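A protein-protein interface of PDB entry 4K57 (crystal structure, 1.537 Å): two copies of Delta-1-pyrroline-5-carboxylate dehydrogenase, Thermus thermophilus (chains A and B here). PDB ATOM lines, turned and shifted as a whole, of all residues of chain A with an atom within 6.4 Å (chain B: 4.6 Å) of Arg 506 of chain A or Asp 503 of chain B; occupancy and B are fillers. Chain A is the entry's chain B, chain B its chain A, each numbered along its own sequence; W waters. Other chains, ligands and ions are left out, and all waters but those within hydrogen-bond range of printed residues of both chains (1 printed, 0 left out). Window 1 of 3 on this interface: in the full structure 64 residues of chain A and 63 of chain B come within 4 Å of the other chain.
Asp 503 of chain A touches Arg 506 of chain B, and with the chains exchanged Arg 506 of chain A touches Asp 503 of chain B.
Positions printed for both chains: 154, 502, 503, 504, 505, 506 and 507.
N of Arg 506 of chain B lies close to OH of Tyr 154 of chain B.
NH2 of Arg 506 of chain A sits at hydrogen-bond distance from O of Leu 509 of chain A, at 2.9 Å.
Of the 8 printed residues of chain B, 2 touch a printed residue of chain A.
Of the 15 printed residues of chain A, 4 touch a printed residue of chain B.
Among the printed residues, Asp or Glu carboxylates within 4 Å of a Lys or Arg side-chain nitrogen of the other chain: Asp 503 of chain A with Arg 506 of chain B and Arg 506 of chain A with Asp 503 of chain B.
Water W1 bridges OH of Tyr 173 of chain A (2.8 Å) and OD1 of Asp 503 of chain B (2.8 Å).
OD2 of Asp 503 of chain B is in hydrogen-bond range of OH of Tyr 173 of chain A (2.7 Å).
The side-chain carboxylate (OD2) of Asp 503 of chain B is in salt-bridge range of the guanidinium group (NH1) of Arg 506 of chain A (2.8 Å).
The side-chain carboxylate (OD2) of Asp 503 of chain A lies within salt-bridge range of the guanidinium group (NH1) of Arg 506 of chain B.
Printed residues of chain B within 4 Å of Tyr 173 of chain A: Asp 503.
Of the printed residues of chain B, Asp 503 of chain A touches Arg 506.
Arg 506 of chain A touches just one residue of chain B: Asp 503 (2.8 Å).
Of the printed residues of chain B, Met 511 of chain A touches Asp 503.
Asp 503 of chain B touches just these residues of chain A: Tyr 173, Arg 506 and Met 511.
Of the printed residues of chain A, Arg 506 of chain B touches Asp 503.
The nearest printed residue of chain B that does not touch Arg 506 of chain A is Arg 506 of chain B (6.0 Å).
Among the printed residues, pairs that only touch across the chains: Met 511 of chain A with Asp 503 of chain B (3.3 Å).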
ATOM      1  N   TYR A 154      25.198  12.550  37.137  1.00  0.00           N
ATOM      2  CA  TYR A 154      25.807  11.504  36.308  1.00  0.00           C
ATOM      3  C   TYR A 154      26.522  10.433  37.123  1.00  0.00           C
ATOM      4  O   TYR A 154      27.042   9.468  36.546  1.00  0.00           O
ATOM      5  CB  TYR A 154      26.783  12.101  35.284  1.00  0.00           C
ATOM      6  CG  TYR A 154      26.102  12.966  34.249  1.00  0.00           C
ATOM      7  CD1 TYR A 154      25.908  14.326  34.467  1.00  0.00           C
ATOM      8  CD2 TYR A 154      25.633  12.418  33.072  1.00  0.00           C
ATOM      9  CE1 TYR A 154      25.264  15.115  33.523  1.00  0.00           C
ATOM     10  CE2 TYR A 154      24.998  13.190  32.127  1.00  0.00           C
ATOM     11  CZ  TYR A 154      24.816  14.539  32.355  1.00  0.00           C
ATOM     12  OH  TYR A 154      24.179  15.299  31.400  1.00  0.00           O
ATOM     13  N   VAL A 159      22.064   5.348  34.708  1.00  0.00           N
ATOM     14  CA  VAL A 159      21.572   4.856  33.426  1.00  0.00           C
ATOM     15  C   VAL A 159      20.454   3.855  33.664  1.00  0.00           C
ATOM     16  O   VAL A 159      20.646   2.859  34.372  1.00  0.00           O
ATOM     17  CB  VAL A 159      22.687   4.166  32.616  1.00  0.00           C
ATOM     18  CG1 VAL A 159      22.163   3.708  31.253  1.00  0.00           C
ATOM     19  CG2 VAL A 159      23.869   5.088  32.450  1.00  0.00           C
ATOM     20  N   TYR A 173      28.839   6.040  33.520  1.00  0.00           N
ATOM     21  CA  TYR A 173      29.589   6.991  32.719  1.00  0.00           C
ATOM     22  C   TYR A 173      31.012   7.094  33.219  1.00  0.00           C
ATOM     23  O   TYR A 173      31.266   6.995  34.426  1.00  0.00           O
ATOM     24  CB  TYR A 173      28.925   8.370  32.762  1.00  0.00           C
ATOM     25  CG  TYR A 173      27.566   8.392  32.126  1.00  0.00           C
ATOM     26  CD1 TYR A 173      26.423   8.570  32.890  1.00  0.00           C
ATOM     27  CD2 TYR A 173      27.422   8.206  30.757  1.00  0.00           C
ATOM     28  CE1 TYR A 173      25.176   8.581  32.309  1.00  0.00           C
ATOM     29  CE2 TYR A 173      26.171   8.207  30.170  1.00  0.00           C
ATOM     30  CZ  TYR A 173      25.062   8.402  30.950  1.00  0.00           C
ATOM     31  OH  TYR A 173      23.820   8.405  30.364  1.00  0.00           O
ATOM     32  N   VAL A 202      33.462  16.312  35.835  1.00  0.00           N
ATOM     33  CA  VAL A 202      33.093  14.905  35.698  1.00  0.00           C
ATOM     34  C   VAL A 202      34.300  13.985  35.479  1.00  0.00           C
ATOM     35  O   VAL A 202      34.137  12.800  35.168  1.00  0.00           O
ATOM     36  CB  VAL A 202      32.021  14.696  34.614  1.00  0.00           C
ATOM     37  CG1 VAL A 202      30.726  15.417  34.996  1.00  0.00           C
ATOM     38  CG2 VAL A 202      32.519  15.160  33.247  1.00  0.00           C
ATOM     39  N   ARG A 286      36.160  14.259  19.911  1.00  0.00           N
ATOM     40  CA  ARG A 286      34.954  15.060  20.041  1.00  0.00           C
ATOM     41  C   ARG A 286      35.350  16.520  19.994  1.00  0.00           C
ATOM     42  O   ARG A 286      36.323  16.919  20.634  1.00  0.00           O
ATOM     43  CB  ARG A 286      34.242  14.766  21.358  1.00  0.00           C
ATOM     44  CG  ARG A 286      33.766  13.329  21.465  1.00  0.00           C
ATOM     45  CD  ARG A 286      32.845  13.152  22.646  1.00  0.00           C
ATOM     46  NE  ARG A 286      32.448  11.751  22.790  1.00  0.00           N
ATOM     47  CZ  ARG A 286      31.685  11.299  23.776  1.00  0.00           C
ATOM     48  NH1 ARG A 286      31.223  12.132  24.699  1.00  0.00           N
ATOM     49  NH2 ARG A 286      31.375  10.014  23.825  1.00  0.00           N
ATOM     50  N   LEU A 502      22.203  20.659  32.198  1.00  0.00           N
ATOM     51  CA  LEU A 502      22.606  19.292  32.528  1.00  0.00           C
ATOM     52  C   LEU A 502      23.244  18.581  31.333  1.00  0.00           C
ATOM     53  O   LEU A 502      24.247  17.861  31.470  1.00  0.00           O
ATOM     54  CB  LEU A 502      21.399  18.504  33.025  1.00  0.00           C
ATOM     55  CG  LEU A 502      20.746  19.011  34.304  1.00  0.00           C
ATOM     56  CD1 LEU A 502      19.538  18.162  34.662  1.00  0.00           C
ATOM     57  CD2 LEU A 502      21.747  19.012  35.431  1.00  0.00           C
ATOM     58  N   ASP A 503      22.685  18.817  30.148  1.00  0.00           N
ATOM     59  CA  ASP A 503      23.171  18.188  28.924  1.00  0.00           C
ATOM     60  C   ASP A 503      24.626  18.502  28.582  1.00  0.00           C
ATOM     61  O   ASP A 503      25.272  17.741  27.875  1.00  0.00           O
ATOM     62  CB  ASP A 503      22.285  18.581  27.739  1.00  0.00           C
ATOM     63  CG  ASP A 503      20.995  17.787  27.677  1.00  0.00           C
ATOM     64  OD1 ASP A 503      20.685  17.026  28.625  1.00  0.00           O
ATOM     65  OD2 ASP A 503      20.276  17.942  26.674  1.00  0.00           O
ATOM     66  N   TYR A 504      25.143  19.630  29.061  1.00  0.00           N
ATOM     67  CA  TYR A 504      26.516  20.004  28.732  1.00  0.00           C
ATOM     68  C   TYR A 504      27.496  18.926  29.167  1.00  0.00           C
ATOM     69  O   TYR A 504      28.414  18.576  28.424  1.00  0.00           O
ATOM     70  CB  TYR A 504      26.866  21.318  29.432  1.00  0.00           C
ATOM     71  CG  TYR A 504      28.111  22.019  28.934  1.00  0.00           C
ATOM     72  CD1 TYR A 504      28.214  22.437  27.608  1.00  0.00           C
ATOM     73  CD2 TYR A 504      29.162  22.298  29.796  1.00  0.00           C
ATOM     74  CE1 TYR A 504      29.340  23.124  27.157  1.00  0.00           C
ATOM     75  CE2 TYR A 504      30.298  22.978  29.350  1.00  0.00           C
ATOM     76  CZ  TYR A 504      30.378  23.385  28.030  1.00  0.00           C
ATOM     77  OH  TYR A 504      31.502  24.080  27.597  1.00  0.00           O
ATOM     78  N   LEU A 505      27.298  18.396  30.365  1.00  0.00           N
ATOM     79  CA  LEU A 505      28.293  17.496  30.934  1.00  0.00           C
ATOM     80  C   LEU A 505      28.339  16.147  30.240  1.00  0.00           C
ATOM     81  O   LEU A 505      29.388  15.514  30.196  1.00  0.00           O
ATOM     82  CB  LEU A 505      28.071  17.317  32.430  1.00  0.00           C
ATOM     83  CG  LEU A 505      28.106  18.612  33.232  1.00  0.00           C
ATOM     84  CD1 LEU A 505      27.965  18.298  34.705  1.00  0.00           C
ATOM     85  CD2 LEU A 505      29.399  19.395  32.970  1.00  0.00           C
ATOM     86  N   ARG A 506      27.204  15.725  29.689  1.00  0.00           N
ATOM     87  CA  ARG A 506      27.121  14.467  28.951  1.00  0.00           C
ATOM     88  C   ARG A 506      28.106  14.423  27.785  1.00  0.00           C
ATOM     89  O   ARG A 506      28.600  13.357  27.398  1.00  0.00           O
ATOM     90  CB  ARG A 506      25.692  14.261  28.444  1.00  0.00           C
ATOM     91  CG  ARG A 506      25.476  12.970  27.670  1.00  0.00           C
ATOM     92  CD  ARG A 506      25.756  11.761  28.547  1.00  0.00           C
ATOM     93  NE  ARG A 506      25.567  10.507  27.819  1.00  0.00           N
ATOM     94  CZ  ARG A 506      26.498   9.915  27.082  1.00  0.00           C
ATOM     95  NH1 ARG A 506      26.226   8.765  26.476  1.00  0.00           N
ATOM     96  NH2 ARG A 506      27.706  10.454  26.960  1.00  0.00           N
ATOM     97  N   LEU A 507      28.398  15.593  27.222  1.00  0.00           N
ATOM     98  CA  LEU A 507      29.358  15.718  26.134  1.00  0.00           C
ATOM     99  C   LEU A 507      30.756  15.236  26.488  1.00  0.00           C
ATOM    100  O   LEU A 507      31.526  14.865  25.604  1.00  0.00           O
ATOM    101  CB  LEU A 507      29.445  17.173  25.676  1.00  0.00           C
ATOM    102  CG  LEU A 507      28.110  17.756  25.228  1.00  0.00           C
ATOM    103  CD1 LEU A 507      28.223  19.254  25.065  1.00  0.00           C
ATOM    104  CD2 LEU A 507      27.649  17.099  23.933  1.00  0.00           C
ATOM    105  N   PHE A 508      31.083  15.247  27.781  1.00  0.00           N
ATOM    106  CA  PHE A 508      32.434  14.936  28.241  1.00  0.00           C
ATOM    107  C   PHE A 508      32.500  13.579  28.923  1.00  0.00           C
ATOM    108  O   PHE A 508      33.416  13.295  29.702  1.00  0.00           O
ATOM    109  CB  PHE A 508      32.920  16.042  29.195  1.00  0.00           C
ATOM    110  CG  PHE A 508      32.579  17.431  28.726  1.00  0.00           C
ATOM    111  CD1 PHE A 508      31.811  18.267  29.524  1.00  0.00           C
ATOM    112  CD2 PHE A 508      33.000  17.884  27.487  1.00  0.00           C
ATOM    113  CE1 PHE A 508      31.483  19.542  29.104  1.00  0.00           C
ATOM    114  CE2 PHE A 508      32.672  19.172  27.055  1.00  0.00           C
ATOM    115  CZ  PHE A 508      31.903  19.983  27.857  1.00  0.00           C
ATOM    116  N   LEU A 509      31.537  12.721  28.595  1.00  0.00           N
ATOM    117  CA  LEU A 509      31.450  11.381  29.172  1.00  0.00           C
ATOM    118  C   LEU A 509      31.217  10.348  28.087  1.00  0.00           C
ATOM    119  O   LEU A 509      30.646  10.659  27.036  1.00  0.00           O
ATOM    120  CB  LEU A 509      30.281  11.312  30.155  1.00  0.00           C
ATOM    121  CG  LEU A 509      30.379  12.174  31.410  1.00  0.00           C
ATOM    122  CD1 LEU A 509      29.040  12.195  32.115  1.00  0.00           C
ATOM    123  CD2 LEU A 509      31.472  11.623  32.328  1.00  0.00           C
ATOM    124  N   GLU A 510      31.675   9.122  28.338  1.00  0.00           N
ATOM    125  CA  GLU A 510      31.279   7.971  27.519  1.00  0.00           C
ATOM    126  C   GLU A 510      30.699   6.916  28.450  1.00  0.00           C
ATOM    127  O   GLU A 510      30.863   7.004  29.667  1.00  0.00           O
ATOM    128  CB  GLU A 510      32.432   7.433  26.662  1.00  0.00           C
ATOM    129  CG  GLU A 510      33.719   7.104  27.408  1.00  0.00           C
ATOM    130  CD  GLU A 510      34.941   7.001  26.480  1.00  0.00           C
ATOM    131  OE1 GLU A 510      34.793   7.024  25.231  1.00  0.00           O
ATOM    132  OE2 GLU A 510      36.064   6.888  27.005  1.00  0.00           O
ATOM    133  N   MET A 511      29.991   5.938  27.892  1.00  0.00           N
ATOM    134  CA  MET A 511      29.265   4.967  28.723  1.00  0.00           C
ATOM    135  C   MET A 511      29.867   3.580  28.592  1.00  0.00           C
ATOM    136  O   MET A 511      30.213   3.140  27.490  1.00  0.00           O
ATOM    137  CB  MET A 511      27.776   4.913  28.348  1.00  0.00           C
ATOM    138  CG  MET A 511      26.906   4.173  29.373  1.00  0.00           C
ATOM    139  SD  MET A 511      25.328   3.599  28.685  1.00  0.00           S
ATOM    140  CE  MET A 511      24.505   5.162  28.406  1.00  0.00           C
ATOM    141  N   TYR B 154      11.697  12.135  25.716  1.00  0.00           N
ATOM    142  CA  TYR B 154      12.196  13.421  25.233  1.00  0.00           C
ATOM    143  C   TYR B 154      11.080  14.406  24.919  1.00  0.00           C
ATOM    144  O   TYR B 154      11.356  15.552  24.556  1.00  0.00           O
ATOM    145  CB  TYR B 154      13.092  13.235  24.006  1.00  0.00           C
ATOM    146  CG  TYR B 154      14.375  12.505  24.316  1.00  0.00           C
ATOM    147  CD1 TYR B 154      14.433  11.120  24.300  1.00  0.00           C
ATOM    148  CD2 TYR B 154      15.518  13.205  24.651  1.00  0.00           C
ATOM    149  CE1 TYR B 154      15.611  10.454  24.600  1.00  0.00           C
ATOM    150  CE2 TYR B 154      16.690  12.558  24.947  1.00  0.00           C
ATOM    151  CZ  TYR B 154      16.732  11.182  24.918  1.00  0.00           C
ATOM    152  OH  TYR B 154      17.908  10.552  25.224  1.00  0.00           O
ATOM    153  N   ALA B 501      19.530   2.169  24.014  1.00  0.00           N
ATOM    154  CA  ALA B 501      19.633   2.922  25.255  1.00  0.00           C
ATOM    155  C   ALA B 501      18.949   4.263  25.064  1.00  0.00           C
ATOM    156  O   ALA B 501      18.905   4.798  23.946  1.00  0.00           O
ATOM    157  CB  ALA B 501      21.103   3.137  25.611  1.00  0.00           C
ATOM    158  N   LEU B 502      18.461   4.834  26.162  1.00  0.00           N
ATOM    159  CA  LEU B 502      17.811   6.136  26.108  1.00  0.00           C
ATOM    160  C   LEU B 502      18.720   7.187  25.456  1.00  0.00           C
ATOM    161  O   LEU B 502      18.256   8.030  24.681  1.00  0.00           O
ATOM    162  CB  LEU B 502      17.416   6.568  27.522  1.00  0.00           C
ATOM    163  CG  LEU B 502      16.355   5.722  28.225  1.00  0.00           C
ATOM    164  CD1 LEU B 502      16.013   6.266  29.606  1.00  0.00           C
ATOM    165  CD2 LEU B 502      15.118   5.661  27.376  1.00  0.00           C
ATOM    166  N   ASP B 503      20.017   7.123  25.760  1.00  0.00           N
ATOM    167  CA  ASP B 503      20.988   8.092  25.263  1.00  0.00           C
ATOM    168  C   ASP B 503      21.093   8.117  23.750  1.00  0.00           C
ATOM    169  O   ASP B 503      21.553   9.088  23.185  1.00  0.00           O
ATOM    170  CB  ASP B 503      22.376   7.804  25.837  1.00  0.00           C
ATOM    171  CG  ASP B 503      22.554   8.333  27.231  1.00  0.00           C
ATOM    172  OD1 ASP B 503      21.559   8.778  27.851  1.00  0.00           O
ATOM    173  OD2 ASP B 503      23.702   8.297  27.704  1.00  0.00           O
ATOM    174  N   TYR B 504      20.690   7.037  23.087  1.00  0.00           N
ATOM    175  CA  TYR B 504      20.815   6.985  21.634  1.00  0.00           C
ATOM    176  C   TYR B 504      20.026   8.092  20.961  1.00  0.00           C
ATOM    177  O   TYR B 504      20.522   8.730  20.043  1.00  0.00           O
ATOM    178  CB  TYR B 504      20.311   5.642  21.118  1.00  0.00           C
ATOM    179  CG  TYR B 504      20.695   5.301  19.695  1.00  0.00           C
ATOM    180  CD1 TYR B 504      22.027   5.177  19.324  1.00  0.00           C
ATOM    181  CD2 TYR B 504      19.719   5.042  18.740  1.00  0.00           C
ATOM    182  CE1 TYR B 504      22.376   4.815  18.020  1.00  0.00           C
ATOM    183  CE2 TYR B 504      20.055   4.680  17.435  1.00  0.00           C
ATOM    184  CZ  TYR B 504      21.388   4.568  17.089  1.00  0.00           C
ATOM    185  OH  TYR B 504      21.723   4.201  15.801  1.00  0.00           O
ATOM    186  N   LEU B 505      18.801   8.308  21.414  1.00  0.00           N
ATOM    187  CA  LEU B 505      17.914   9.233  20.724  1.00  0.00           C
ATOM    188  C   LEU B 505      18.366  10.676  20.872  1.00  0.00           C
ATOM    189  O   LEU B 505      18.095  11.498  20.002  1.00  0.00           O
ATOM    190  CB  LEU B 505      16.475   9.068  21.208  1.00  0.00           C
ATOM    191  CG  LEU B 505      15.919   7.653  21.037  1.00  0.00           C
ATOM    192  CD1 LEU B 505      14.454   7.585  21.449  1.00  0.00           C
ATOM    193  CD2 LEU B 505      16.108   7.154  19.605  1.00  0.00           C
ATOM    194  N   ARG B 506      19.061  10.979  21.967  1.00  0.00           N
ATOM    195  CA  ARG B 506      19.567  12.330  22.204  1.00  0.00           C
ATOM    196  C   ARG B 506      20.516  12.795  21.094  1.00  0.00           C
ATOM    197  O   ARG B 506      20.620  13.987  20.802  1.00  0.00           O
ATOM    198  CB  ARG B 506      20.271  12.392  23.566  1.00  0.00           C
ATOM    199  CG  ARG B 506      20.805  13.768  23.956  1.00  0.00           C
ATOM    200  CD  ARG B 506      19.697  14.799  24.014  1.00  0.00           C
ATOM    201  NE  ARG B 506      20.207  16.125  24.375  1.00  0.00           N
ATOM    202  CZ  ARG B 506      20.660  17.015  23.499  1.00  0.00           C
ATOM    203  NH1 ARG B 506      21.087  18.206  23.918  1.00  0.00           N
ATOM    204  NH2 ARG B 506      20.673  16.725  22.201  1.00  0.00           N
ATOM    205  N   LEU B 507      21.200  11.843  20.476  1.00  0.00           N
ATOM    206  CA  LEU B 507      22.104  12.117  19.371  1.00  0.00           C
ATOM    207  C   LEU B 507      21.404  12.750  18.169  1.00  0.00           C
ATOM    208  O   LEU B 507      22.035  13.421  17.358  1.00  0.00           O
ATOM    209  CB  LEU B 507      22.759  10.813  18.920  1.00  0.00           C
ATOM    210  CG  LEU B 507      23.544  10.092  20.012  1.00  0.00           C
ATOM    211  CD1 LEU B 507      24.000   8.740  19.500  1.00  0.00           C
ATOM    212  CD2 LEU B 507      24.723  10.948  20.453  1.00  0.00           C
HETATM  213  O   HOH W   1      21.158   7.494  30.331  1.00  0.00           O
